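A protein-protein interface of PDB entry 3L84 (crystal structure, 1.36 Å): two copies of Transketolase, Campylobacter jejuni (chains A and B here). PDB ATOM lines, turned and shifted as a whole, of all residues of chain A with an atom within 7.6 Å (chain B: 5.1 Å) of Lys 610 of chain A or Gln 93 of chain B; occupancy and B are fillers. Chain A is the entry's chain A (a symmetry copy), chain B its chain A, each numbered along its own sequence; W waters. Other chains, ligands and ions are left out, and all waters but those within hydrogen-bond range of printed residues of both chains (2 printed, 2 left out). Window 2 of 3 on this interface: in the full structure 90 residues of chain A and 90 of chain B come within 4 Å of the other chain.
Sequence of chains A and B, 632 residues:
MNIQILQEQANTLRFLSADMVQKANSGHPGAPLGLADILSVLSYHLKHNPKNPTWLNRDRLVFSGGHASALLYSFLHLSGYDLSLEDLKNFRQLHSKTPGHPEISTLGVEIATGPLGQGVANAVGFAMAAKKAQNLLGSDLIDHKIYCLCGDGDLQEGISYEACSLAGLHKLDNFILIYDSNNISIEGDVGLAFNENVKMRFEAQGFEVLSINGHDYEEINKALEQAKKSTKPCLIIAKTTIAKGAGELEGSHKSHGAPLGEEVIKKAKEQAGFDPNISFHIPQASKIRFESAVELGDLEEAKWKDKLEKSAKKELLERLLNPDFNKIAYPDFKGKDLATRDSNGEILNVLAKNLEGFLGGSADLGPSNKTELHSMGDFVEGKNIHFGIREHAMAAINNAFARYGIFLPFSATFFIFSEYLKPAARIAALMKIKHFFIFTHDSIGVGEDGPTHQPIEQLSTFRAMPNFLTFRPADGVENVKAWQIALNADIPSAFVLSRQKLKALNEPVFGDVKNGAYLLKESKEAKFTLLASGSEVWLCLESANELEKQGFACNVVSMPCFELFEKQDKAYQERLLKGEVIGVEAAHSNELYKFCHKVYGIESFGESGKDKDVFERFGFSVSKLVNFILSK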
ATOM      1  N   ILE A 444       7.998 -18.401 -10.928  1.00  0.00           N
ATOM      2  CA  ILE A 444       8.590 -19.144 -12.057  1.00  0.00           C
ATOM      3  C   ILE A 444       8.505 -20.650 -11.866  1.00  0.00           C
ATOM      4  O   ILE A 444       8.651 -21.376 -12.848  1.00  0.00           O
ATOM      5  CB  ILE A 444      10.074 -18.752 -12.287  1.00  0.00           C
ATOM      6  CG1 ILE A 444      10.910 -18.748 -10.983  1.00  0.00           C
ATOM      7  CG2 ILE A 444      10.152 -17.376 -12.949  1.00  0.00           C
ATOM      8  CD1 ILE A 444      12.451 -18.812 -11.216  1.00  0.00           C
ATOM      9  N   GLY A 445       8.240 -21.136 -10.651  1.00  0.00           N
ATOM     10  CA  GLY A 445       7.991 -22.554 -10.421  1.00  0.00           C
ATOM     11  C   GLY A 445       6.791 -23.097 -11.180  1.00  0.00           C
ATOM     12  O   GLY A 445       6.641 -24.321 -11.337  1.00  0.00           O
ATOM     13  N   VAL A 446       5.939 -22.211 -11.688  1.00  0.00           N
ATOM     14  CA  VAL A 446       4.907 -22.588 -12.655  1.00  0.00           C
ATOM     15  C   VAL A 446       5.461 -23.414 -13.826  1.00  0.00           C
ATOM     16  O   VAL A 446       4.826 -24.365 -14.303  1.00  0.00           O
ATOM     17  CB  VAL A 446       4.206 -21.295 -13.145  1.00  0.00           C
ATOM     18  CG1 VAL A 446       3.456 -21.512 -14.468  1.00  0.00           C
ATOM     19  CG2 VAL A 446       3.247 -20.818 -12.070  1.00  0.00           C
ATOM     20  N   GLY A 447       6.638 -23.053 -14.311  1.00  0.00           N
ATOM     21  CA  GLY A 447       7.319 -23.834 -15.334  1.00  0.00           C
ATOM     22  C   GLY A 447       6.835 -23.570 -16.741  1.00  0.00           C
ATOM     23  O   GLY A 447       6.959 -22.480 -17.267  1.00  0.00           O
ATOM     24  N   GLU A 448       6.315 -24.598 -17.388  1.00  0.00           N
ATOM     25  CA  GLU A 448       6.171 -24.614 -18.837  1.00  0.00           C
ATOM     26  C   GLU A 448       5.205 -23.571 -19.407  1.00  0.00           C
ATOM     27  O   GLU A 448       5.372 -23.139 -20.556  1.00  0.00           O
ATOM     28  CB  GLU A 448       5.757 -26.008 -19.336  1.00  0.00           C
ATOM     29  CG  GLU A 448       6.855 -27.100 -19.181  1.00  0.00           C
ATOM     30  CD  GLU A 448       6.834 -27.836 -17.877  1.00  0.00           C
ATOM     31  OE1 GLU A 448       6.294 -27.352 -16.859  1.00  0.00           O
ATOM     32  OE2 GLU A 448       7.370 -28.975 -17.911  1.00  0.00           O
ATOM     33  N   ASP A 449       4.195 -23.172 -18.655  1.00  0.00           N
ATOM     34  CA  ASP A 449       3.304 -22.146 -19.155  1.00  0.00           C
ATOM     35  C   ASP A 449       4.027 -20.849 -19.511  1.00  0.00           C
ATOM     36  O   ASP A 449       3.533 -20.089 -20.361  1.00  0.00           O
ATOM     37  CB  ASP A 449       2.169 -21.864 -18.196  1.00  0.00           C
ATOM     38  CG  ASP A 449       1.062 -22.867 -18.261  1.00  0.00           C
ATOM     39  OD1 ASP A 449       0.977 -23.700 -19.192  1.00  0.00           O
ATOM     40  OD2 ASP A 449       0.200 -22.809 -17.351  1.00  0.00           O
ATOM     41  N   GLN A 454       3.947 -16.468 -15.099  1.00  0.00           N
ATOM     42  CA  GLN A 454       4.915 -16.509 -14.010  1.00  0.00           C
ATOM     43  C   GLN A 454       4.947 -15.184 -13.335  1.00  0.00           C
ATOM     44  O   GLN A 454       5.440 -14.210 -13.925  1.00  0.00           O
ATOM     45  CB  GLN A 454       6.284 -16.892 -14.525  1.00  0.00           C
ATOM     46  CG  GLN A 454       6.335 -18.380 -14.961  1.00  0.00           C
ATOM     47  CD  GLN A 454       7.537 -18.732 -15.797  1.00  0.00           C
ATOM     48  OE1 GLN A 454       8.280 -17.852 -16.208  1.00  0.00           O
ATOM     49  NE2 GLN A 454       7.753 -20.012 -16.066  1.00  0.00           N
ATOM     50  N   GLU A 607      10.620 -17.663 -18.054  1.00  0.00           N
ATOM     51  CA  GLU A 607      10.911 -18.494 -19.213  1.00  0.00           C
ATOM     52  C   GLU A 607       9.985 -19.698 -19.209  1.00  0.00           C
ATOM     53  O   GLU A 607       9.686 -20.246 -18.186  1.00  0.00           O
ATOM     54  CB  GLU A 607      12.358 -18.991 -19.142  1.00  0.00           C
ATOM     55  CG  GLU A 607      13.428 -17.932 -19.355  1.00  0.00           C
ATOM     56  CD  GLU A 607      13.541 -17.444 -20.768  1.00  0.00           C
ATOM     57  OE1 GLU A 607      12.921 -17.999 -21.708  1.00  0.00           O
ATOM     58  OE2 GLU A 607      14.285 -16.432 -20.932  1.00  0.00           O
ATOM     59  N   SER A 608       9.586 -20.160 -20.389  1.00  0.00           N
ATOM     60  CA  SER A 608       8.882 -21.421 -20.534  1.00  0.00           C
ATOM     61  C   SER A 608       9.855 -22.583 -20.476  1.00  0.00           C
ATOM     62  O   SER A 608      10.682 -22.751 -21.361  1.00  0.00           O
ATOM     63  CB  SER A 608       8.092 -21.396 -21.867  1.00  0.00           C
ATOM     64  OG  SER A 608       7.479 -22.637 -22.115  1.00  0.00           O
ATOM     65  N   GLY A 609       9.727 -23.441 -19.479  1.00  0.00           N
ATOM     66  CA  GLY A 609      10.564 -24.633 -19.342  1.00  0.00           C
ATOM     67  C   GLY A 609      10.159 -25.397 -18.107  1.00  0.00           C
ATOM     68  O   GLY A 609       9.304 -24.953 -17.341  1.00  0.00           O
ATOM     69  N   LYS A 610      10.730 -26.588 -17.924  1.00  0.00           N
ATOM     70  CA  LYS A 610      10.472 -27.355 -16.698  1.00  0.00           C
ATOM     71  C   LYS A 610      10.856 -26.551 -15.482  1.00  0.00           C
ATOM     72  O   LYS A 610      11.870 -25.853 -15.514  1.00  0.00           O
ATOM     73  CB  LYS A 610      11.277 -28.647 -16.762  1.00  0.00           C
ATOM     74  CG  LYS A 610      10.869 -29.642 -17.878  1.00  0.00           C
ATOM     75  CD  LYS A 610      11.762 -30.886 -17.865  1.00  0.00           C
ATOM     76  CE  LYS A 610      11.457 -31.801 -19.064  1.00  0.00           C
ATOM     77  NZ  LYS A 610      10.043 -32.236 -19.146  1.00  0.00           N
ATOM     78  N   ASP A 611      10.073 -26.624 -14.414  1.00  0.00           N
ATOM     79  CA  ASP A 611      10.324 -25.875 -13.208  1.00  0.00           C
ATOM     80  C   ASP A 611      11.773 -25.922 -12.739  1.00  0.00           C
ATOM     81  O   ASP A 611      12.358 -24.874 -12.469  1.00  0.00           O
ATOM     82  CB  ASP A 611       9.334 -26.264 -12.091  1.00  0.00           C
ATOM     83  CG  ASP A 611       9.337 -27.742 -11.705  1.00  0.00           C
ATOM     84  OD1 ASP A 611      10.082 -28.595 -12.237  1.00  0.00           O
ATOM     85  OD2 ASP A 611       8.502 -28.029 -10.803  1.00  0.00           O
ATOM     86  N   LYS A 612      12.340 -27.110 -12.663  1.00  0.00           N
ATOM     87  CA  LYS A 612      13.721 -27.224 -12.161  1.00  0.00           C
ATOM     88  C   LYS A 612      14.701 -26.487 -13.094  1.00  0.00           C
ATOM     89  O   LYS A 612      15.663 -25.878 -12.613  1.00  0.00           O
ATOM     90  CB  LYS A 612      14.127 -28.679 -11.925  1.00  0.00           C
ATOM     91  CG  LYS A 612      13.444 -29.326 -10.719  1.00  0.00           C
ATOM     92  CD  LYS A 612      13.839 -30.804 -10.628  1.00  0.00           C
ATOM     93  CE  LYS A 612      13.120 -31.564  -9.508  1.00  0.00           C
ATOM     94  NZ  LYS A 612      13.528 -33.017  -9.486  1.00  0.00           N
ATOM     95  N   ASP A 613      14.455 -26.526 -14.398  1.00  0.00           N
ATOM     96  CA  ASP A 613      15.306 -25.833 -15.370  1.00  0.00           C
ATOM     97  C   ASP A 613      15.185 -24.303 -15.227  1.00  0.00           C
ATOM     98  O   ASP A 613      16.180 -23.582 -15.275  1.00  0.00           O
ATOM     99  CB  ASP A 613      14.927 -26.205 -16.798  1.00  0.00           C
ATOM    100  CG  ASP A 613      15.205 -27.660 -17.161  1.00  0.00           C
ATOM    101  OD1 ASP A 613      15.899 -28.362 -16.372  1.00  0.00           O
ATOM    102  OD2 ASP A 613      14.725 -28.065 -18.272  1.00  0.00           O
ATOM    103  N   VAL A 614      13.960 -23.835 -14.975  1.00  0.00           N
ATOM    104  CA  VAL A 614      13.701 -22.411 -14.852  1.00  0.00           C
ATOM    105  C   VAL A 614      14.329 -21.894 -13.537  1.00  0.00           C
ATOM    106  O   VAL A 614      14.964 -20.852 -13.527  1.00  0.00           O
ATOM    107  CB  VAL A 614      12.195 -22.086 -14.984  1.00  0.00           C
ATOM    108  CG1 VAL A 614      11.933 -20.594 -14.809  1.00  0.00           C
ATOM    109  CG2 VAL A 614      11.722 -22.542 -16.346  1.00  0.00           C
ATOM    110  N   PHE A 615      14.164 -22.612 -12.430  1.00  0.00           N
ATOM    111  CA  PHE A 615      14.786 -22.146 -11.203  1.00  0.00           C
ATOM    112  C   PHE A 615      16.306 -22.071 -11.341  1.00  0.00           C
ATOM    113  O   PHE A 615      16.900 -21.120 -10.862  1.00  0.00           O
ATOM    114  CB  PHE A 615      14.387 -23.030 -10.003  1.00  0.00           C
ATOM    115  CG  PHE A 615      13.085 -22.648  -9.330  1.00  0.00           C
ATOM    116  CD1 PHE A 615      12.927 -21.419  -8.735  1.00  0.00           C
ATOM    117  CD2 PHE A 615      12.046 -23.550  -9.264  1.00  0.00           C
ATOM    118  CE1 PHE A 615      11.719 -21.093  -8.092  1.00  0.00           C
ATOM    119  CE2 PHE A 615      10.844 -23.199  -8.621  1.00  0.00           C
ATOM    120  CZ  PHE A 615      10.710 -22.005  -8.042  1.00  0.00           C
ATOM    121  N   GLU A 616      16.909 -23.038 -12.020  1.00  0.00           N
ATOM    122  CA  GLU A 616      18.372 -23.035 -12.197  1.00  0.00           C
ATOM    123  C   GLU A 616      18.773 -21.838 -13.060  1.00  0.00           C
ATOM    124  O   GLU A 616      19.733 -21.119 -12.751  1.00  0.00           O
ATOM    125  CB  GLU A 616      18.852 -24.354 -12.828  1.00  0.00           C
ATOM    126  CG  GLU A 616      20.344 -24.460 -12.992  1.00  0.00           C
ATOM    127  CD  GLU A 616      21.102 -24.476 -11.688  1.00  0.00           C
ATOM    128  OE1 GLU A 616      20.608 -25.011 -10.659  1.00  0.00           O
ATOM    129  OE2 GLU A 616      22.259 -23.999 -11.695  1.00  0.00           O
ATOM    130  N   ARG A 617      18.035 -21.610 -14.143  1.00  0.00           N
ATOM    131  CA  ARG A 617      18.292 -20.488 -15.034  1.00  0.00           C
ATOM    132  C   ARG A 617      18.332 -19.155 -14.274  1.00  0.00           C
ATOM    133  O   ARG A 617      19.158 -18.294 -14.574  1.00  0.00           O
ATOM    134  CB  ARG A 617      17.183 -20.496 -16.109  1.00  0.00           C
ATOM    135  CG  ARG A 617      16.992 -19.202 -16.861  1.00  0.00           C
ATOM    136  CD  ARG A 617      18.107 -18.894 -17.824  1.00  0.00           C
ATOM    137  NE  ARG A 617      17.562 -17.846 -18.692  1.00  0.00           N
ATOM    138  CZ  ARG A 617      17.445 -16.563 -18.362  1.00  0.00           C
ATOM    139  NH1 ARG A 617      17.948 -16.088 -17.240  1.00  0.00           N
ATOM    140  NH2 ARG A 617      16.803 -15.764 -19.188  1.00  0.00           N
ATOM    141  N   ALA B  24       6.519 -33.135 -24.542  1.00  0.00           N
ATOM    142  CA  ALA B  24       6.788 -32.202 -23.447  1.00  0.00           C
ATOM    143  C   ALA B  24       6.242 -32.704 -22.107  1.00  0.00           C
ATOM    144  O   ALA B  24       6.613 -32.181 -21.049  1.00  0.00           O
ATOM    145  CB  ALA B  24       6.172 -30.824 -23.761  1.00  0.00           C
ATOM    146  N   ASN B  90      10.807 -29.410 -29.310  1.00  0.00           N
ATOM    147  CA  ASN B  90      11.311 -28.668 -28.160  1.00  0.00           C
ATOM    148  C   ASN B  90      10.192 -27.853 -27.488  1.00  0.00           C
ATOM    149  O   ASN B  90      10.475 -26.940 -26.696  1.00  0.00           O
ATOM    150  CB  ASN B  90      12.435 -27.722 -28.604  1.00  0.00           C
ATOM    151  CG  ASN B  90      13.657 -28.465 -29.081  1.00  0.00           C
ATOM    152  OD1 ASN B  90      13.855 -29.636 -28.731  1.00  0.00           O
ATOM    153  ND2 ASN B  90      14.469 -27.811 -29.884  1.00  0.00           N
ATOM    154  N   PHE B  91       8.933 -28.151 -27.799  1.00  0.00           N
ATOM    155  CA  PHE B  91       7.820 -27.465 -27.203  1.00  0.00           C
ATOM    156  C   PHE B  91       7.942 -27.416 -25.677  1.00  0.00           C
ATOM    157  O   PHE B  91       8.217 -28.407 -25.020  1.00  0.00           O
ATOM    158  CB  PHE B  91       6.546 -28.196 -27.625  1.00  0.00           C
ATOM    159  CG  PHE B  91       5.245 -27.612 -27.122  1.00  0.00           C
ATOM    160  CD1 PHE B  91       4.841 -26.320 -27.471  1.00  0.00           C
ATOM    161  CD2 PHE B  91       4.369 -28.367 -26.348  1.00  0.00           C
ATOM    162  CE1 PHE B  91       3.599 -25.833 -27.088  1.00  0.00           C
ATOM    163  CE2 PHE B  91       3.133 -27.881 -25.974  1.00  0.00           C
ATOM    164  CZ  PHE B  91       2.751 -26.621 -26.348  1.00  0.00           C
ATOM    165  N   ARG B  92       7.754 -26.230 -25.159  1.00  0.00           N
ATOM    166  CA  ARG B  92       7.713 -25.978 -23.717  1.00  0.00           C
ATOM    167  C   ARG B  92       9.033 -26.216 -22.979  1.00  0.00           C
ATOM    168  O   ARG B  92       9.064 -26.237 -21.761  1.00  0.00           O
ATOM    169  CB  ARG B  92       6.544 -26.701 -23.034  1.00  0.00           C
ATOM    170  CG  ARG B  92       5.196 -26.025 -23.272  1.00  0.00           C
ATOM    171  CD  ARG B  92       3.966 -26.873 -22.804  1.00  0.00           C
ATOM    172  NE  ARG B  92       2.840 -25.970 -22.810  1.00  0.00           N
ATOM    173  CZ  ARG B  92       2.309 -25.338 -21.770  1.00  0.00           C
ATOM    174  NH1 ARG B  92       2.593 -25.687 -20.538  1.00  0.00           N
ATOM    175  NH2 ARG B  92       1.461 -24.336 -21.978  1.00  0.00           N
ATOM    176  N   GLN B  93      10.122 -26.325 -23.707  1.00  0.00           N
ATOM    177  CA  GLN B  93      11.445 -26.543 -23.108  1.00  0.00           C
ATOM    178  C   GLN B  93      12.232 -25.233 -23.022  1.00  0.00           C
ATOM    179  O   GLN B  93      12.119 -24.354 -23.899  1.00  0.00           O
ATOM    180  CB  GLN B  93      12.242 -27.577 -23.876  1.00  0.00           C
ATOM    181  CG  GLN B  93      11.546 -28.932 -23.981  1.00  0.00           C
ATOM    182  CD  GLN B  93      10.902 -29.357 -22.685  1.00  0.00           C
ATOM    183  OE1 GLN B  93       9.650 -29.455 -22.577  1.00  0.00           O
ATOM    184  NE2 GLN B  93      11.705 -29.510 -21.653  1.00  0.00           N
ATOM    185  N   LEU B  94      13.078 -25.138 -21.997  1.00  0.00           N
ATOM    186  CA  LEU B  94      13.813 -23.919 -21.753  1.00  0.00           C
ATOM    187  C   LEU B  94      14.569 -23.471 -22.985  1.00  0.00           C
ATOM    188  O   LEU B  94      15.311 -24.239 -23.595  1.00  0.00           O
ATOM    189  CB  LEU B  94      14.780 -24.100 -20.600  1.00  0.00           C
ATOM    190  CG  LEU B  94      15.497 -22.864 -20.111  1.00  0.00           C
ATOM    191  CD1 LEU B  94      14.464 -21.974 -19.390  1.00  0.00           C
ATOM    192  CD2 LEU B  94      16.652 -23.238 -19.169  1.00  0.00           C
ATOM    193  N   HIS B  95      14.342 -22.205 -23.341  1.00  0.00           N
ATOM    194  CA  HIS B  95      14.991 -21.485 -24.424  1.00  0.00           C
ATOM    195  C   HIS B  95      14.618 -21.935 -25.819  1.00  0.00           C
ATOM    196  O   HIS B  95      15.260 -21.528 -26.798  1.00  0.00           O
ATOM    197  CB  HIS B  95      16.505 -21.399 -24.219  1.00  0.00           C
ATOM    198  CG  HIS B  95      16.902 -20.777 -22.896  1.00  0.00           C
ATOM    199  ND1 HIS B  95      17.922 -21.275 -22.114  1.00  0.00           N
ATOM    200  CD2 HIS B  95      16.354 -19.753 -22.190  1.00  0.00           C
ATOM    201  CE1 HIS B  95      18.026 -20.553 -21.011  1.00  0.00           C
ATOM    202  NE2 HIS B  95      17.073 -19.636 -21.017  1.00  0.00           N
ATOM    203  N   SER B  96      13.550 -22.695 -25.952  1.00  0.00           N
ATOM    204  CA  SER B  96      13.089 -23.096 -27.291  1.00  0.00           C
ATOM    205  C   SER B  96      12.344 -21.970 -28.000  1.00  0.00           C
ATOM    206  O   SER B  96      11.922 -21.007 -27.366  1.00  0.00           O
ATOM    207  CB  SER B  96      12.213 -24.329 -27.246  1.00  0.00           C
ATOM    208  OG  SER B  96      10.872 -24.007 -26.959  1.00  0.00           O
ATOM    209  N   THR B  98       9.457 -22.539 -29.171  1.00  0.00           N
ATOM    210  CA  THR B  98       8.079 -22.995 -29.017  1.00  0.00           C
ATOM    211  C   THR B  98       7.659 -22.989 -27.552  1.00  0.00           C
ATOM    212  O   THR B  98       7.313 -24.017 -26.985  1.00  0.00           O
ATOM    213  CB  THR B  98       7.932 -24.385 -29.648  1.00  0.00           C
ATOM    214  OG1 THR B  98       9.029 -25.187 -29.179  1.00  0.00           O
ATOM    215  CG2 THR B  98       7.965 -24.286 -31.176  1.00  0.00           C
HETATM  216  O   HOH W   1      12.287 -20.556 -22.399  1.00  0.00           O
HETATM  217  O   HOH W   2      10.059 -22.556 -24.544  1.00  0.00           O
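No position is printed for both chains.
The backbone carbonyl oxygen (O) of Ser 608 of chain A sits close to the backbone NH (N) of Leu 94 of chain B.
The backbone carbonyl oxygen (O) of Ser 608 of chain A sits close to the backbone carbonyl oxygen (O) of Gln 93 of chain B (3.3 Å).
A ring nitrogen (NE2) of His 95 of chain B sits at hydrogen-bond distance from the guanidinium group of Arg 617 of chain A (3.0 Å).
NH1 of Arg 92 of chain B is in salt-bridge range of OD1 of Asp 449 of chain A, at 2.9 Å.
Arg 92 of chain B touches Glu 448 of chain A (NH1 to CB, 3.4 Å).
CB of Glu 607 of chain A touches CD1 of Leu 94 of chain B (3.7 Å).
OE1 of Glu 607 of chain A touches CD2 of His 95 of chain B (3.9 Å).
Ser 608 of chain A touches Arg 92 of chain B (OG to CA, 3.7 Å).
O of Arg 92 of chain B touches CA of Gly 609 of chain A, 3.3 Å away.
Leu 94 of chain B touches Gly 609 of chain A.
NZ of Lys 610 of chain A touches O of Ala 24 of chain B, at 3.9 Å.
NE2 of Gln 93 of chain B touches CE of Lys 610 of chain A (3.5 Å).
Leu 94 of chain B touches Asp 613 of chain A.
O of Gln 93 of chain B is in hydrogen-bond range of OG of Ser 96 of chain B (3.3 Å).
The backbone carbonyl oxygen (O) of Gly 609 of chain A sits at hydrogen-bond distance from the backbone NH (N) of Glu 448 of chain A.
OE2 of Glu 607 of chain A is in salt-bridge range of NH2 of Arg 617 of chain A (3.1 Å).
The backbone carbonyl oxygen of Glu 448 of chain A is in hydrogen-bond range of the side-chain hydroxyl of Ser 608 of chain A.
The backbone carbonyl oxygen (O) of Glu 607 of chain A is in hydrogen-bond range of the side-chain amide nitrogen (NE2) of Gln 454 of chain A, 2.9 Å away.
The backbone NH of Arg 92 of chain B is in hydrogen-bond range of the backbone carbonyl oxygen of Thr 98 of chain B.
Water W1 lies within hydrogen-bond range of OE1 of Glu 607 of chain A (2.7 Å), N of His 95 of chain B (2.8 Å) and O of Ser 608 of chain A (2.9 Å).
Water W2 lies within hydrogen-bond range of O of Gln 93 of chain B (2.8 Å), OG of Ser 96 of chain B (2.9 Å) and O of Ser 608 of chain A (3.2 Å).
Of the 9 printed residues of chain B, 5 touch a printed residue of chain A.
Hydrophobic or aromatic side chains of chain B that line the printed part of chain A: Leu 94 and His 95.
Along chain A the printed residues that touch a printed residue of chain B span positions 448 to 617.
Among the printed residues, Asp or Glu carboxylates within 4 Å of a Lys or Arg side-chain nitrogen of the other chain: Asp 449 of chain A with Arg 92 of chain B (2.9 Å).
Of the printed residues of chain B, Glu 448 of chain A touches Arg 92 (3.4 Å).
Of the printed residues of chain B, Glu 607 of chain A touches Leu 94 (3.7 Å) and His 95 (3.9 Å).
Of the printed residues of chain B, Ser 608 of chain A touches Arg 92 (3.7 Å), Gln 93 (3.3 Å) and Leu 94 (3.4 Å).
Of the printed residues of chain B, Gly 609 of chain A touches Arg 92 and Leu 94.
Printed residues of chain B within 4 Å of Lys 610 of chain A: Ala 24 (3.9 Å) and Gln 93 (3.5 Å).
Gln 93 of chain B touches just these residues of chain A: Ser 608 (3.3 Å) and Lys 610 (3.5 Å).
Printed residues of chain A within 4 Å of His 95 of chain B: Glu 607 (3.9 Å) and Arg 617 (3.0 Å).
The nearest residue of chain B that does not touch Lys 610 of chain A is Arg 92 of chain B (4.2 Å).
The nearest residue of chain A that does not touch Gln 93 of chain B is Gly 609 of chain A (4.1 Å).
The nearest printed residue of chain B that does not touch Gly 609 of chain A is Gln 93 of chain B (4.1 Å).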
